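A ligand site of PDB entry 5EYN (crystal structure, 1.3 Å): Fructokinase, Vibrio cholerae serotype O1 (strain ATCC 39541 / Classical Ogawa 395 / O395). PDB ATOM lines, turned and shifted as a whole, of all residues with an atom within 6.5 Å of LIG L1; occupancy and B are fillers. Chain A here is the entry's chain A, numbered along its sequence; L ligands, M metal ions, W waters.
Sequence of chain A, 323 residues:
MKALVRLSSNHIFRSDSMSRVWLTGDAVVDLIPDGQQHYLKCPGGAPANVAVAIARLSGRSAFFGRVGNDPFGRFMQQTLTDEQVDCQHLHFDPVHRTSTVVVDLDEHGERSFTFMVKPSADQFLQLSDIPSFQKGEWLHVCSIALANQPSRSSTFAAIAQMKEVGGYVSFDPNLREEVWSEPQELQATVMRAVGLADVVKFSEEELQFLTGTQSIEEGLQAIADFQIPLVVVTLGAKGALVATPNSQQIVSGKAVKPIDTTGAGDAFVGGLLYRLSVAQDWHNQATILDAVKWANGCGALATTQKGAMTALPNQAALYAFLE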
ATOM      1  N   ASP A  26       7.164  26.419 -32.769  1.00  0.00           N
ATOM      2  CA  ASP A  26       7.829  26.464 -31.469  1.00  0.00           C
ATOM      3  C   ASP A  26       7.746  25.152 -30.713  1.00  0.00           C
ATOM      4  O   ASP A  26       6.669  24.708 -30.371  1.00  0.00           O
ATOM      5  CB  ASP A  26       7.251  27.583 -30.602  1.00  0.00           C
ATOM      6  CG  ASP A  26       5.749  27.482 -30.352  1.00  0.00           C
ATOM      7  OD1 ASP A  26       5.331  27.711 -29.175  1.00  0.00           O
ATOM      8  OD2 ASP A  26       4.969  27.229 -31.305  1.00  0.00           O
ATOM      9  N   VAL A  28       8.775  23.939 -27.091  1.00  0.00           N
ATOM     10  CA  VAL A  28       8.935  24.698 -25.871  1.00  0.00           C
ATOM     11  C   VAL A  28       8.994  23.773 -24.680  1.00  0.00           C
ATOM     12  O   VAL A  28       8.482  22.667 -24.727  1.00  0.00           O
ATOM     13  CB  VAL A  28       7.791  25.681 -25.637  1.00  0.00           C
ATOM     14  CG1 VAL A  28       7.335  26.356 -26.940  1.00  0.00           C
ATOM     15  CG2 VAL A  28       6.641  25.067 -24.937  1.00  0.00           C
ATOM     16  N   VAL A  29       9.615  24.261 -23.617  1.00  0.00           N
ATOM     17  CA  VAL A  29       9.490  23.597 -22.328  1.00  0.00           C
ATOM     18  C   VAL A  29       8.391  24.282 -21.529  1.00  0.00           C
ATOM     19  O   VAL A  29       8.474  25.477 -21.242  1.00  0.00           O
ATOM     20  CB  VAL A  29      10.826  23.549 -21.550  1.00  0.00           C
ATOM     21  CG1 VAL A  29      10.605  23.119 -20.115  1.00  0.00           C
ATOM     22  CG2 VAL A  29      11.813  22.618 -22.248  1.00  0.00           C
ATOM     23  N   ASP A  30       7.362  23.501 -21.218  1.00  0.00           N
ATOM     24  CA  ASP A  30       6.282  23.943 -20.350  1.00  0.00           C
ATOM     25  C   ASP A  30       6.620  23.555 -18.910  1.00  0.00           C
ATOM     26  O   ASP A  30       6.824  22.375 -18.579  1.00  0.00           O
ATOM     27  CB  ASP A  30       4.954  23.261 -20.732  1.00  0.00           C
ATOM     28  CG  ASP A  30       4.355  23.752 -22.047  1.00  0.00           C
ATOM     29  OD1 ASP A  30       4.560  24.922 -22.423  1.00  0.00           O
ATOM     30  OD2 ASP A  30       3.602  22.956 -22.648  1.00  0.00           O
ATOM     31  N   PRO A  43       7.820  18.559 -21.998  1.00  0.00           N
ATOM     32  CA  PRO A  43       7.979  18.972 -23.396  1.00  0.00           C
ATOM     33  C   PRO A  43       6.668  19.483 -23.926  1.00  0.00           C
ATOM     34  O   PRO A  43       5.596  18.941 -23.618  1.00  0.00           O
ATOM     35  CB  PRO A  43       8.400  17.685 -24.089  1.00  0.00           C
ATOM     36  CG  PRO A  43       7.788  16.584 -23.237  1.00  0.00           C
ATOM     37  CD  PRO A  43       7.838  17.090 -21.831  1.00  0.00           C
ATOM     38  N   GLY A  44       6.731  20.516 -24.745  1.00  0.00           N
ATOM     39  CA  GLY A  44       5.531  21.135 -25.253  1.00  0.00           C
ATOM     40  C   GLY A  44       5.839  21.955 -26.488  1.00  0.00           C
ATOM     41  O   GLY A  44       6.838  21.742 -27.180  1.00  0.00           O
ATOM     42  N   GLY A  45       4.935  22.881 -26.757  1.00  0.00           N
ATOM     43  CA  GLY A  45       4.978  23.703 -27.954  1.00  0.00           C
ATOM     44  C   GLY A  45       4.006  23.119 -28.965  1.00  0.00           C
ATOM     45  O   GLY A  45       4.177  21.987 -29.405  1.00  0.00           O
ATOM     46  N   ALA A  46       2.993  23.880 -29.353  1.00  0.00           N
ATOM     47  CA  ALA A  46       1.876  23.310 -30.098  1.00  0.00           C
ATOM     48  C   ALA A  46       2.281  22.472 -31.311  1.00  0.00           C
ATOM     49  O   ALA A  46       1.827  21.353 -31.448  1.00  0.00           O
ATOM     50  CB  ALA A  46       0.867  24.370 -30.482  1.00  0.00           C
ATOM     51  N   PRO A  47       3.124  22.998 -32.219  1.00  0.00           N
ATOM     52  CA  PRO A  47       3.442  22.148 -33.365  1.00  0.00           C
ATOM     53  C   PRO A  47       4.243  20.889 -32.984  1.00  0.00           C
ATOM     54  O   PRO A  47       4.107  19.848 -33.628  1.00  0.00           O
ATOM     55  CB  PRO A  47       4.242  23.065 -34.288  1.00  0.00           C
ATOM     56  CG  PRO A  47       4.720  24.141 -33.440  1.00  0.00           C
ATOM     57  CD  PRO A  47       3.728  24.335 -32.343  1.00  0.00           C
ATOM     58  N   ASN A  49       3.783  19.270 -30.154  1.00  0.00           N
ATOM     59  CA  ASN A  49       2.728  18.436 -29.597  1.00  0.00           C
ATOM     60  C   ASN A  49       1.997  17.721 -30.710  1.00  0.00           C
ATOM     61  O   ASN A  49       1.723  16.515 -30.618  1.00  0.00           O
ATOM     62  CB  ASN A  49       1.737  19.304 -28.817  1.00  0.00           C
ATOM     63  CG  ASN A  49       2.348  19.967 -27.602  1.00  0.00           C
ATOM     64  OD1 ASN A  49       3.344  19.510 -27.056  1.00  0.00           O
ATOM     65  ND2 ASN A  49       1.718  21.046 -27.160  1.00  0.00           N
ATOM     66  N   SER A  99      12.126  28.565 -26.177  1.00  0.00           N
ATOM     67  CA  SER A  99      10.934  29.035 -25.505  1.00  0.00           C
ATOM     68  C   SER A  99      10.691  28.267 -24.202  1.00  0.00           C
ATOM     69  O   SER A  99      10.764  27.037 -24.161  1.00  0.00           O
ATOM     70  CB  SER A  99       9.737  28.879 -26.424  1.00  0.00           C
ATOM     71  OG  SER A  99       8.577  29.376 -25.786  1.00  0.00           O
ATOM     72  N   VAL A 101       7.886  28.300 -21.006  1.00  0.00           N
ATOM     73  CA  VAL A 101       6.553  28.762 -20.703  1.00  0.00           C
ATOM     74  C   VAL A 101       6.161  28.274 -19.315  1.00  0.00           C
ATOM     75  O   VAL A 101       6.333  27.097 -18.975  1.00  0.00           O
ATOM     76  CB  VAL A 101       5.572  28.217 -21.751  1.00  0.00           C
ATOM     77  CG1 VAL A 101       4.135  28.534 -21.370  1.00  0.00           C
ATOM     78  CG2 VAL A 101       5.891  28.810 -23.119  1.00  0.00           C
ATOM     79  N   VAL A 103       3.160  27.515 -16.776  1.00  0.00           N
ATOM     80  CA  VAL A 103       1.736  27.201 -16.825  1.00  0.00           C
ATOM     81  C   VAL A 103       1.040  27.454 -15.482  1.00  0.00           C
ATOM     82  O   VAL A 103       1.551  27.071 -14.433  1.00  0.00           O
ATOM     83  CB  VAL A 103       1.506  25.739 -17.252  1.00  0.00           C
ATOM     84  CG1 VAL A 103       0.034  25.398 -17.335  1.00  0.00           C
ATOM     85  CG2 VAL A 103       2.204  25.450 -18.576  1.00  0.00           C
ATOM     86  N   GLY A 109      -5.952  27.343 -21.468  1.00  0.00           N
ATOM     87  CA  GLY A 109      -5.478  27.829 -22.752  1.00  0.00           C
ATOM     88  C   GLY A 109      -4.593  29.039 -22.614  1.00  0.00           C
ATOM     89  O   GLY A 109      -3.770  29.128 -21.712  1.00  0.00           O
ATOM     90  N   PHE A 113      -0.827  30.539 -19.805  1.00  0.00           N
ATOM     91  CA  PHE A 113       0.593  30.543 -20.165  1.00  0.00           C
ATOM     92  C   PHE A 113       1.257  31.893 -19.971  1.00  0.00           C
ATOM     93  O   PHE A 113       0.696  32.924 -20.299  1.00  0.00           O
ATOM     94  CB  PHE A 113       0.765  30.161 -21.633  1.00  0.00           C
ATOM     95  CG  PHE A 113       0.173  28.823 -21.977  1.00  0.00           C
ATOM     96  CD1 PHE A 113      -0.877  28.743 -22.869  1.00  0.00           C
ATOM     97  CD2 PHE A 113       0.675  27.653 -21.438  1.00  0.00           C
ATOM     98  CE1 PHE A 113      -1.429  27.520 -23.191  1.00  0.00           C
ATOM     99  CE2 PHE A 113       0.125  26.417 -21.775  1.00  0.00           C
ATOM    100  CZ  PHE A 113      -0.928  26.357 -22.644  1.00  0.00           C
ATOM    101  N   PHE A 115       4.884  33.410 -21.258  1.00  0.00           N
ATOM    102  CA  PHE A 115       6.053  33.177 -22.089  1.00  0.00           C
ATOM    103  C   PHE A 115       7.254  33.924 -21.548  1.00  0.00           C
ATOM    104  O   PHE A 115       7.274  35.162 -21.532  1.00  0.00           O
ATOM    105  CB  PHE A 115       5.749  33.591 -23.533  1.00  0.00           C
ATOM    106  CG  PHE A 115       4.785  32.649 -24.187  1.00  0.00           C
ATOM    107  CD1 PHE A 115       5.235  31.672 -25.044  1.00  0.00           C
ATOM    108  CD2 PHE A 115       3.434  32.700 -23.882  1.00  0.00           C
ATOM    109  CE1 PHE A 115       4.357  30.764 -25.598  1.00  0.00           C
ATOM    110  CE2 PHE A 115       2.558  31.799 -24.443  1.00  0.00           C
ATOM    111  CZ  PHE A 115       3.007  30.828 -25.292  1.00  0.00           C
ATOM    112  N   ILE A 144       1.961  31.385 -33.392  1.00  0.00           N
ATOM    113  CA  ILE A 144       3.195  31.869 -32.815  1.00  0.00           C
ATOM    114  C   ILE A 144       4.254  31.975 -33.918  1.00  0.00           C
ATOM    115  O   ILE A 144       5.112  32.861 -33.883  1.00  0.00           O
ATOM    116  CB  ILE A 144       3.644  31.012 -31.633  1.00  0.00           C
ATOM    117  CG1 ILE A 144       2.931  31.487 -30.381  1.00  0.00           C
ATOM    118  CG2 ILE A 144       5.171  31.082 -31.423  1.00  0.00           C
ATOM    119  CD1 ILE A 144       3.282  30.705 -29.128  1.00  0.00           C
ATOM    120  N   ASN A 174      -4.307  29.088 -32.451  1.00  0.00           N
ATOM    121  CA  ASN A 174      -3.643  28.801 -31.191  1.00  0.00           C
ATOM    122  C   ASN A 174      -3.052  30.093 -30.618  1.00  0.00           C
ATOM    123  O   ASN A 174      -1.841  30.222 -30.385  1.00  0.00           O
ATOM    124  CB  ASN A 174      -2.542  27.756 -31.401  1.00  0.00           C
ATOM    125  CG  ASN A 174      -2.655  26.604 -30.455  1.00  0.00           C
ATOM    126  OD1 ASN A 174      -3.329  26.693 -29.419  1.00  0.00           O
ATOM    127  ND2 ASN A 174      -2.040  25.501 -30.836  1.00  0.00           N
ATOM    128  N   ARG A 176      -1.652  33.218 -28.817  1.00  0.00           N
ATOM    129  CA  ARG A 176      -0.884  33.569 -27.645  1.00  0.00           C
ATOM    130  C   ARG A 176      -0.396  35.010 -27.845  1.00  0.00           C
ATOM    131  O   ARG A 176       0.716  35.247 -28.321  1.00  0.00           O
ATOM    132  CB  ARG A 176       0.301  32.607 -27.463  1.00  0.00           C
ATOM    133  CG  ARG A 176      -0.070  31.119 -27.465  1.00  0.00           C
ATOM    134  CD  ARG A 176      -0.790  30.661 -26.217  1.00  0.00           C
ATOM    135  NE  ARG A 176      -0.918  29.218 -26.274  1.00  0.00           N
ATOM    136  CZ  ARG A 176      -1.920  28.558 -26.833  1.00  0.00           C
ATOM    137  NH1 ARG A 176      -2.969  29.174 -27.323  1.00  0.00           N
ATOM    138  NH2 ARG A 176      -1.884  27.231 -26.870  1.00  0.00           N
ATOM    139  N   THR A 262      -3.757  21.363 -20.884  1.00  0.00           N
ATOM    140  CA  THR A 262      -2.672  21.900 -21.711  1.00  0.00           C
ATOM    141  C   THR A 262      -2.497  21.059 -22.959  1.00  0.00           C
ATOM    142  O   THR A 262      -2.257  19.851 -22.868  1.00  0.00           O
ATOM    143  CB  THR A 262      -1.330  21.882 -20.945  1.00  0.00           C
ATOM    144  OG1 THR A 262      -1.430  22.669 -19.750  1.00  0.00           O
ATOM    145  CG2 THR A 262      -0.197  22.465 -21.781  1.00  0.00           C
ATOM    146  N   GLY A 263      -2.585  21.693 -24.122  1.00  0.00           N
ATOM    147  CA  GLY A 263      -2.371  20.954 -25.348  1.00  0.00           C
ATOM    148  C   GLY A 263      -3.477  20.012 -25.815  1.00  0.00           C
ATOM    149  O   GLY A 263      -3.259  19.296 -26.793  1.00  0.00           O
ATOM    150  N   ALA A 264      -4.636  19.972 -25.142  1.00  0.00           N
ATOM    151  CA  ALA A 264      -5.738  19.137 -25.609  1.00  0.00           C
ATOM    152  C   ALA A 264      -6.103  19.451 -27.065  1.00  0.00           C
ATOM    153  O   ALA A 264      -6.410  18.590 -27.872  1.00  0.00           O
ATOM    154  CB  ALA A 264      -6.966  19.309 -24.729  1.00  0.00           C
ATOM    155  N   GLY A 265      -6.003  20.723 -27.421  1.00  0.00           N
ATOM    156  CA  GLY A 265      -6.345  21.169 -28.764  1.00  0.00           C
ATOM    157  C   GLY A 265      -5.340  20.631 -29.769  1.00  0.00           C
ATOM    158  O   GLY A 265      -5.704  20.364 -30.910  1.00  0.00           O
ATOM    159  N   ASP A 266      -4.086  20.484 -29.354  1.00  0.00           N
ATOM    160  CA  ASP A 266      -3.040  19.982 -30.240  1.00  0.00           C
ATOM    161  C   ASP A 266      -3.198  18.481 -30.437  1.00  0.00           C
ATOM    162  O   ASP A 266      -2.956  17.963 -31.522  1.00  0.00           O
ATOM    163  CB  ASP A 266      -1.666  20.291 -29.695  1.00  0.00           C
ATOM    164  CG  ASP A 266      -1.445  21.776 -29.464  1.00  0.00           C
ATOM    165  OD1 ASP A 266      -2.022  22.581 -30.250  1.00  0.00           O
ATOM    166  OD2 ASP A 266      -0.708  22.097 -28.509  1.00  0.00           O
ATOM    167  N   ALA A 308       1.498  18.482 -22.125  1.00  0.00           N
ATOM    168  CA  ALA A 308       0.801  18.389 -23.398  1.00  0.00           C
ATOM    169  C   ALA A 308       0.987  17.046 -24.079  1.00  0.00           C
ATOM    170  O   ALA A 308       0.092  16.563 -24.757  1.00  0.00           O
ATOM    171  CB  ALA A 308       1.255  19.498 -24.326  1.00  0.00           C
HETATM  172  C1  LIG L   1       2.687  27.478 -27.176  1.00  0.00           C
HETATM  173  C2  LIG L   1       1.945  26.694 -26.109  1.00  0.00           C
HETATM  174  C3  LIG L   1       2.760  25.706 -25.284  1.00  0.00           C
HETATM  175  C4  LIG L   1       1.850  24.549 -25.069  1.00  0.00           C
HETATM  176  C5  LIG L   1       0.984  24.610 -26.283  1.00  0.00           C
HETATM  177  C6  LIG L   1      -0.424  24.124 -26.057  1.00  0.00           C
HETATM  178  O1  LIG L   1       3.136  26.642 -28.199  1.00  0.00           O
HETATM  179  O2  LIG L   1       1.379  27.634 -25.257  1.00  0.00           O
HETATM  180  O3  LIG L   1       3.188  26.371 -24.129  1.00  0.00           O
HETATM  181  O4  LIG L   1       2.506  23.316 -25.022  1.00  0.00           O
HETATM  182  O5  LIG L   1       0.960  25.947 -26.749  1.00  0.00           O
HETATM  183  O6  LIG L   1      -1.202  24.230 -27.220  1.00  0.00           O
HETATM  184 BE1  LG2 L   2      -4.470  23.741 -26.438  1.00  0.00          BE
HETATM  185  F1  LG2 L   2      -4.249  23.715 -24.916  1.00  0.00           F
HETATM  186  F2  LG2 L   2      -3.569  22.732 -27.209  1.00  0.00           F
HETATM  187  F3  LG2 L   2      -4.026  25.061 -27.045  1.00  0.00           F
HETATM  188 CA    CA M   1      -5.277  25.628 -28.745  1.00  0.00          CA
HETATM  189  O   HOH W   1       2.222  27.523 -30.817  1.00  0.00           O
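Merely in contact with LIG L1: Val 28, Gly 44, Val 101, Phe 113, Phe 115, Ile 144, Asn 174 and Gly 263. Hydrophobic or aromatic side chains that line LIG L1: Val 28, Ala 46, Val 101, Phe 113, Phe 115 and Ile 144. Within 4 Å of LIG L1: Asp 26, Val 28, Asp 30, Gly 44, Gly 45, Ala 46, Asn 49, Val 101, Phe 113, Phe 115, Ile 144, Asn 174, Arg 176, Gly 263 and Asp 266.
The backbone NH (N) of Gly 44 is in hydrogen-bond range of the backbone carbonyl oxygen (O) of Val 28, at 2.8 Å. The side-chain carboxylate of Asp 266 lies within hydrogen-bond range of the side-chain amide nitrogen of Asn 49, 3.0 Å away. NH1 of Arg 176 sits close to O of Asn 174 (3.4 Å). The side-chain carboxylate of Asp 266 sits at hydrogen-bond distance from the side-chain amide nitrogen of Asn 174, at 3.0 Å. The backbone carbonyl oxygen (O) of Val 29 sits at hydrogen-bond distance from the backbone NH (N) of Val 101. The side-chain amide nitrogen (ND2) of Asn 49 sits close to the backbone carbonyl oxygen (O) of Gly 45, 3.5 Å away.
The guanidinium group (NE) of Arg 176 sits at hydrogen-bond distance from an oxygen (O2) of LIG L1 (3.0 Å). A fluorine (F2) of LG2 L2 lies within hydrogen-bond range of the backbone NH of Asp 266. The backbone NH (N) of Gly 265 sits at hydrogen-bond distance from a fluorine (F2) of LG2 L2 (3.2 Å). An oxygen (O6) of LIG L1 is in hydrogen-bond range of the side-chain carboxylate (OD2) of Asp 266 (2.5 Å). An oxygen (O1) of LIG L1 sits at hydrogen-bond distance from the backbone NH (N) of Ala 46, at 3.0 Å. The guanidinium group of Arg 176 lies close to a fluorine (F3) of LG2 L2 (3.1 Å). A fluorine (F1) of LG2 L2 sits at hydrogen-bond distance from the backbone NH (N) of Gly 263, 2.7 Å away. The side-chain carboxylate (OD1) of Asp 30 is in hydrogen-bond range of an oxygen (O3) of LIG L1 (2.6 Å). ND2 of Asn 49 lies within hydrogen-bond range of O4 of LIG L1, 3.2 Å away. An oxygen (O4) of LIG L1 lies within hydrogen-bond range of the backbone NH (N) of Gly 45 (3.0 Å). The side-chain carboxylate (OD1) of Asp 26 sits at hydrogen-bond distance from an oxygen (O1) of LIG L1 (2.6 Å).
An oxygen (O6) of LIG L1 sits at hydrogen-bond distance from a fluorine (F2) of LG2 L2.
Water W1 bridges the side-chain carboxylate of Asp 26 and an oxygen (O1) of LIG L1.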
